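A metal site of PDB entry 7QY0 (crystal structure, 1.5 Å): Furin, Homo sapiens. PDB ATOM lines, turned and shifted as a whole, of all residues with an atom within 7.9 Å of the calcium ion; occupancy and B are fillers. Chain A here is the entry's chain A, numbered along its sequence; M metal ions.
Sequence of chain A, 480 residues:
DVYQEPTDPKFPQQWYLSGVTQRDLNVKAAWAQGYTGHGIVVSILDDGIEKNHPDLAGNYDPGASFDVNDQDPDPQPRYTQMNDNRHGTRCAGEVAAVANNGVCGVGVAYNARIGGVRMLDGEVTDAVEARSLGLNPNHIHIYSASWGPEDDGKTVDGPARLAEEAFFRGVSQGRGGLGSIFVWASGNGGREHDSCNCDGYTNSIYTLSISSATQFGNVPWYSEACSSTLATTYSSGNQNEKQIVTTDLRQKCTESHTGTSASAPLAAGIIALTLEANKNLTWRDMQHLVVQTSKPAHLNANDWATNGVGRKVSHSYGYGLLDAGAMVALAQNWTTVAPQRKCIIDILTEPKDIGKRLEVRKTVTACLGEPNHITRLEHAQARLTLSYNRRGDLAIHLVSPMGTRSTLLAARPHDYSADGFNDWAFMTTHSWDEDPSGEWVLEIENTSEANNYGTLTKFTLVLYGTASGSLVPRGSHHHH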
ATOM      1  N   PRO A   6      24.338  21.580  -8.474  1.00  0.00           N
ATOM      2  CA  PRO A   6      24.976  20.265  -8.376  1.00  0.00           C
ATOM      3  C   PRO A   6      26.227  20.297  -7.519  1.00  0.00           C
ATOM      4  O   PRO A   6      26.976  21.272  -7.497  1.00  0.00           O
ATOM      5  CB  PRO A   6      25.315  19.918  -9.825  1.00  0.00           C
ATOM      6  CG  PRO A   6      24.304  20.685 -10.640  1.00  0.00           C
ATOM      7  CD  PRO A   6      24.056  21.958  -9.878  1.00  0.00           C
ATOM      8  N   THR A   7      26.468  19.177  -6.837  1.00  0.00           N
ATOM      9  CA  THR A   7      27.613  19.013  -5.962  1.00  0.00           C
ATOM     10  C   THR A   7      28.751  18.238  -6.619  1.00  0.00           C
ATOM     11  O   THR A   7      29.769  18.012  -5.981  1.00  0.00           O
ATOM     12  CB  THR A   7      27.154  18.297  -4.696  1.00  0.00           C
ATOM     13  OG1 THR A   7      26.586  17.045  -5.074  1.00  0.00           O
ATOM     14  CG2 THR A   7      26.105  19.131  -3.957  1.00  0.00           C
ATOM     15  N   ASP A   8      28.608  17.881  -7.887  1.00  0.00           N
ATOM     16  CA  ASP A   8      29.599  17.042  -8.536  1.00  0.00           C
ATOM     17  C   ASP A   8      30.983  17.694  -8.504  1.00  0.00           C
ATOM     18  O   ASP A   8      31.106  18.921  -8.593  1.00  0.00           O
ATOM     19  CB  ASP A   8      29.172  16.766  -9.972  1.00  0.00           C
ATOM     20  CG  ASP A   8      27.787  16.147 -10.042  1.00  0.00           C
ATOM     21  OD1 ASP A   8      26.828  16.829  -9.616  1.00  0.00           O
ATOM     22  OD2 ASP A   8      27.670  14.994 -10.487  1.00  0.00           O
ATOM     23  N   PRO A   9      32.032  16.879  -8.384  1.00  0.00           N
ATOM     24  CA  PRO A   9      33.369  17.448  -8.114  1.00  0.00           C
ATOM     25  C   PRO A   9      33.870  18.358  -9.216  1.00  0.00           C
ATOM     26  O   PRO A   9      34.582  19.322  -8.927  1.00  0.00           O
ATOM     27  CB  PRO A   9      34.265  16.213  -7.939  1.00  0.00           C
ATOM     28  CG  PRO A   9      33.499  15.073  -8.600  1.00  0.00           C
ATOM     29  CD  PRO A   9      32.045  15.410  -8.382  1.00  0.00           C
ATOM     30  N   LYS A  10      33.501  18.125 -10.480  1.00  0.00           N
ATOM     31  CA  LYS A  10      33.973  18.998 -11.549  1.00  0.00           C
ATOM     32  C   LYS A  10      32.915  19.974 -12.031  1.00  0.00           C
ATOM     33  O   LYS A  10      33.147  20.675 -13.012  1.00  0.00           O
ATOM     34  CB  LYS A  10      34.500  18.167 -12.703  1.00  0.00           C
ATOM     35  CG  LYS A  10      35.690  17.375 -12.266  1.00  0.00           C
ATOM     36  CD  LYS A  10      36.219  16.534 -13.384  1.00  0.00           C
ATOM     37  N   PHE A  11      31.780  20.080 -11.329  1.00  0.00           N
ATOM     38  CA  PHE A  11      30.789  21.062 -11.767  1.00  0.00           C
ATOM     39  C   PHE A  11      31.349  22.475 -11.736  1.00  0.00           C
ATOM     40  O   PHE A  11      31.054  23.246 -12.669  1.00  0.00           O
ATOM     41  CB  PHE A  11      29.517  21.002 -10.920  1.00  0.00           C
ATOM     42  CG  PHE A  11      28.524  22.087 -11.260  1.00  0.00           C
ATOM     43  CD1 PHE A  11      27.925  22.135 -12.507  1.00  0.00           C
ATOM     44  CD2 PHE A  11      28.210  23.065 -10.339  1.00  0.00           C
ATOM     45  CE1 PHE A  11      27.028  23.135 -12.831  1.00  0.00           C
ATOM     46  CE2 PHE A  11      27.308  24.071 -10.656  1.00  0.00           C
ATOM     47  CZ  PHE A  11      26.720  24.110 -11.903  1.00  0.00           C
ATOM     48  N   GLN A  14      32.800  23.446 -15.009  1.00  0.00           N
ATOM     49  CA  GLN A  14      31.897  23.563 -16.157  1.00  0.00           C
ATOM     50  C   GLN A  14      31.448  25.020 -16.288  1.00  0.00           C
ATOM     51  O   GLN A  14      30.284  25.387 -16.076  1.00  0.00           O
ATOM     52  CB  GLN A  14      30.747  22.579 -15.997  1.00  0.00           C
ATOM     53  CG  GLN A  14      31.265  21.129 -15.978  1.00  0.00           C
ATOM     54  CD  GLN A  14      30.170  20.077 -15.914  1.00  0.00           C
ATOM     55  OE1 GLN A  14      29.408  20.008 -14.957  1.00  0.00           O
ATOM     56  NE2 GLN A  14      30.126  19.222 -16.931  1.00  0.00           N
ATOM     57  N   HIS A  53      29.431   3.734 -18.163  1.00  0.00           N
ATOM     58  CA  HIS A  53      30.169   4.816 -17.524  1.00  0.00           C
ATOM     59  C   HIS A  53      29.488   5.215 -16.222  1.00  0.00           C
ATOM     60  O   HIS A  53      28.263   5.409 -16.219  1.00  0.00           O
ATOM     61  CB  HIS A  53      30.293   6.026 -18.458  1.00  0.00           C
ATOM     62  CG  HIS A  53      31.328   7.016 -18.021  1.00  0.00           C
ATOM     63  ND1 HIS A  53      31.168   7.802 -16.893  1.00  0.00           N
ATOM     64  CD2 HIS A  53      32.544   7.318 -18.523  1.00  0.00           C
ATOM     65  CE1 HIS A  53      32.240   8.560 -16.737  1.00  0.00           C
ATOM     66  NE2 HIS A  53      33.097   8.287 -17.713  1.00  0.00           N
ATOM     67  N   PRO A  54      30.220   5.351 -15.106  1.00  0.00           N
ATOM     68  CA  PRO A  54      29.557   5.705 -13.844  1.00  0.00           C
ATOM     69  C   PRO A  54      28.741   6.987 -13.893  1.00  0.00           C
ATOM     70  O   PRO A  54      27.842   7.158 -13.062  1.00  0.00           O
ATOM     71  CB  PRO A  54      30.733   5.838 -12.856  1.00  0.00           C
ATOM     72  CG  PRO A  54      31.815   4.979 -13.424  1.00  0.00           C
ATOM     73  CD  PRO A  54      31.660   5.079 -14.938  1.00  0.00           C
ATOM     74  N   ASP A  55      29.014   7.904 -14.825  1.00  0.00           N
ATOM     75  CA  ASP A  55      28.227   9.130 -14.927  1.00  0.00           C
ATOM     76  C   ASP A  55      27.175   9.064 -16.028  1.00  0.00           C
ATOM     77  O   ASP A  55      26.447  10.043 -16.212  1.00  0.00           O
ATOM     78  CB  ASP A  55      29.124  10.366 -15.137  1.00  0.00           C
ATOM     79  CG  ASP A  55      28.785  11.521 -14.173  1.00  0.00           C
ATOM     80  OD1 ASP A  55      28.188  11.263 -13.116  1.00  0.00           O
ATOM     81  OD2 ASP A  55      29.124  12.691 -14.477  1.00  0.00           O
ATOM     82  N   LEU A  56      27.072   7.951 -16.762  1.00  0.00           N
ATOM     83  CA  LEU A  56      26.032   7.773 -17.776  1.00  0.00           C
ATOM     84  C   LEU A  56      25.026   6.676 -17.443  1.00  0.00           C
ATOM     85  O   LEU A  56      23.865   6.765 -17.847  1.00  0.00           O
ATOM     86  CB  LEU A  56      26.643   7.457 -19.145  1.00  0.00           C
ATOM     87  CG  LEU A  56      27.594   8.516 -19.691  1.00  0.00           C
ATOM     88  CD1 LEU A  56      28.159   8.012 -21.019  1.00  0.00           C
ATOM     89  CD2 LEU A  56      26.923   9.859 -19.861  1.00  0.00           C
ATOM     90  N   ALA A  96      23.762  14.627 -20.770  1.00  0.00           N
ATOM     91  CA  ALA A  96      22.997  13.964 -19.723  1.00  0.00           C
ATOM     92  C   ALA A  96      23.843  13.227 -18.694  1.00  0.00           C
ATOM     93  O   ALA A  96      23.361  12.245 -18.099  1.00  0.00           O
ATOM     94  CB  ALA A  96      21.998  12.973 -20.333  1.00  0.00           C
ATOM     95  N   ALA A  97      25.054  13.680 -18.405  1.00  0.00           N
ATOM     96  CA  ALA A  97      25.768  13.096 -17.281  1.00  0.00           C
ATOM     97  C   ALA A  97      24.967  13.282 -15.988  1.00  0.00           C
ATOM     98  O   ALA A  97      24.342  14.327 -15.758  1.00  0.00           O
ATOM     99  CB  ALA A  97      27.153  13.728 -17.120  1.00  0.00           C
ATOM    100  N   VAL A  98      25.013  12.258 -15.146  1.00  0.00           N
ATOM    101  CA  VAL A  98      24.217  12.228 -13.912  1.00  0.00           C
ATOM    102  C   VAL A  98      24.713  13.287 -12.950  1.00  0.00           C
ATOM    103  O   VAL A  98      25.917  13.555 -12.850  1.00  0.00           O
ATOM    104  CB  VAL A  98      24.321  10.825 -13.288  1.00  0.00           C
ATOM    105  CG1 VAL A  98      23.695  10.787 -11.908  1.00  0.00           C
ATOM    106  CG2 VAL A  98      23.684   9.803 -14.224  1.00  0.00           C
ATOM    107  N   ALA A  99      23.781  13.889 -12.219  1.00  0.00           N
ATOM    108  CA  ALA A  99      24.068  14.954 -11.272  1.00  0.00           C
ATOM    109  C   ALA A  99      24.056  14.438  -9.831  1.00  0.00           C
ATOM    110  O   ALA A  99      23.335  13.503  -9.503  1.00  0.00           O
ATOM    111  CB  ALA A  99      23.037  16.084 -11.401  1.00  0.00           C
ATOM    112  N   ASN A 100      24.879  15.075  -9.001  1.00  0.00           N
ATOM    113  CA  ASN A 100      24.859  14.885  -7.539  1.00  0.00           C
ATOM    114  C   ASN A 100      25.233  13.460  -7.144  1.00  0.00           C
ATOM    115  O   ASN A 100      24.748  12.917  -6.147  1.00  0.00           O
ATOM    116  CB  ASN A 100      23.504  15.296  -6.971  1.00  0.00           C
ATOM    117  CG  ASN A 100      23.208  16.777  -7.177  1.00  0.00           C
ATOM    118  OD1 ASN A 100      23.997  17.633  -6.784  1.00  0.00           O
ATOM    119  ND2 ASN A 100      22.094  17.087  -7.831  1.00  0.00           N
ATOM    120  N   ASN A 101      26.164  12.868  -7.897  1.00  0.00           N
ATOM    121  CA  ASN A 101      26.600  11.498  -7.667  1.00  0.00           C
ATOM    122  C   ASN A 101      28.103  11.379  -7.417  1.00  0.00           C
ATOM    123  O   ASN A 101      28.644  10.283  -7.474  1.00  0.00           O
ATOM    124  CB  ASN A 101      26.185  10.602  -8.841  1.00  0.00           C
ATOM    125  CG  ASN A 101      26.972  10.898 -10.126  1.00  0.00           C
ATOM    126  OD1 ASN A 101      27.494  11.992 -10.328  1.00  0.00           O
ATOM    127  ND2 ASN A 101      27.040   9.900 -11.001  1.00  0.00           N
ATOM    128  N   GLY A 102      28.787  12.490  -7.139  1.00  0.00           N
ATOM    129  CA  GLY A 102      30.195  12.457  -6.792  1.00  0.00           C
ATOM    130  C   GLY A 102      31.144  12.106  -7.916  1.00  0.00           C
ATOM    131  O   GLY A 102      32.317  11.824  -7.651  1.00  0.00           O
ATOM    132  N   VAL A 103      30.683  12.136  -9.162  1.00  0.00           N
ATOM    133  CA  VAL A 103      31.453  11.713 -10.326  1.00  0.00           C
ATOM    134  C   VAL A 103      31.457  12.837 -11.358  1.00  0.00           C
ATOM    135  O   VAL A 103      30.402  13.388 -11.682  1.00  0.00           O
ATOM    136  CB  VAL A 103      30.880  10.418 -10.949  1.00  0.00           C
ATOM    137  CG1 VAL A 103      31.658  10.064 -12.211  1.00  0.00           C
ATOM    138  CG2 VAL A 103      30.885   9.272  -9.936  1.00  0.00           C
ATOM    139  N   CYS A 104      32.660  13.191 -11.836  1.00  0.00           N
ATOM    140  CA  CYS A 104      32.853  14.177 -12.903  1.00  0.00           C
ATOM    141  C   CYS A 104      31.954  15.388 -12.720  1.00  0.00           C
ATOM    142  O   CYS A 104      31.934  15.985 -11.641  1.00  0.00           O
ATOM    143  CB  CYS A 104      32.650  13.498 -14.260  1.00  0.00           C
ATOM    144  SG  CYS A 104      33.438  14.292 -15.711  1.00  0.00           S
ATOM    145  N   GLY A 105      31.226  15.791 -13.770  1.00  0.00           N
ATOM    146  CA  GLY A 105      30.355  16.945 -13.669  1.00  0.00           C
ATOM    147  C   GLY A 105      28.908  16.580 -13.893  1.00  0.00           C
ATOM    148  O   GLY A 105      28.469  15.524 -13.415  1.00  0.00           O
ATOM    149  N   VAL A 106      28.153  17.415 -14.624  1.00  0.00           N
ATOM    150  CA  VAL A 106      26.751  17.120 -14.922  1.00  0.00           C
ATOM    151  C   VAL A 106      26.457  17.411 -16.388  1.00  0.00           C
ATOM    152  O   VAL A 106      27.145  18.174 -17.047  1.00  0.00           O
ATOM    153  CB  VAL A 106      25.755  17.930 -14.056  1.00  0.00           C
ATOM    154  CG1 VAL A 106      26.074  17.810 -12.593  1.00  0.00           C
ATOM    155  CG2 VAL A 106      25.729  19.403 -14.471  1.00  0.00           C
ATOM    156  N   GLY A 107      25.377  16.804 -16.870  1.00  0.00           N
ATOM    157  CA  GLY A 107      24.841  17.165 -18.163  1.00  0.00           C
ATOM    158  C   GLY A 107      23.978  18.410 -18.091  1.00  0.00           C
ATOM    159  O   GLY A 107      23.491  18.804 -17.029  1.00  0.00           O
ATOM    160  N   TYR A 110      20.421  16.875 -17.032  1.00  0.00           N
ATOM    161  CA  TYR A 110      20.988  15.773 -16.251  1.00  0.00           C
ATOM    162  C   TYR A 110      19.942  14.764 -15.782  1.00  0.00           C
ATOM    163  O   TYR A 110      20.336  13.772 -15.163  1.00  0.00           O
ATOM    164  CB  TYR A 110      21.810  16.294 -15.069  1.00  0.00           C
ATOM    165  CG  TYR A 110      21.114  17.241 -14.107  1.00  0.00           C
ATOM    166  CD1 TYR A 110      20.138  16.778 -13.243  1.00  0.00           C
ATOM    167  CD2 TYR A 110      21.495  18.572 -14.022  1.00  0.00           C
ATOM    168  CE1 TYR A 110      19.522  17.631 -12.341  1.00  0.00           C
ATOM    169  CE2 TYR A 110      20.878  19.436 -13.129  1.00  0.00           C
ATOM    170  CZ  TYR A 110      19.895  18.951 -12.284  1.00  0.00           C
ATOM    171  OH  TYR A 110      19.272  19.784 -11.373  1.00  0.00           O
ATOM    172  N   THR A 247      32.297  13.385 -19.441  1.00  0.00           N
ATOM    173  CA  THR A 247      32.631  11.974 -19.343  1.00  0.00           C
ATOM    174  C   THR A 247      33.583  11.557 -20.462  1.00  0.00           C
ATOM    175  O   THR A 247      33.490  12.044 -21.588  1.00  0.00           O
ATOM    176  CB  THR A 247      31.363  11.148 -19.424  1.00  0.00           C
ATOM    177  OG1 THR A 247      30.563  11.596 -20.545  1.00  0.00           O
ATOM    178  CG2 THR A 247      30.553  11.298 -18.170  1.00  0.00           C
HETATM  179 CA    CA M   1      28.129  13.501 -12.224  1.00  0.00          CA
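Within 4 Å of the calcium ion: Asp 8, Asp 55, Val 98, Asn 101, Val 103 and Gly 105. Along chain A the residues within 4 Å of the calcium ion span positions 8 to 105. The nearest printed residue that does not touch the calcium ion is Cys 104 (4.3 Å).
OD1 of Asp 8 lies within hydrogen-bond range of N of Asn 100, 2.7 Å away. The backbone NH (N) of Asp 55 lies within hydrogen-bond range of a ring nitrogen (ND1) of His 53 (3.0 Å).
The calcium ion is bound by O of Val 98, 2.3 Å away. OD2 of Asp 8 binds the calcium ion (2.3 Å). The calcium ion is bound by the backbone carbonyl oxygen (O) of Val 103, 2.3 Å away. The calcium ion is bound by O of Gly 105 (2.4 Å). The side-chain carboxylate (OD1) of Asp 55 binds the calcium ion (2.4 Å). OD1 of Asn 101 is bound to the calcium ion. The calcium ion is bound by the side-chain carboxylate (OD2) of Asp 55.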
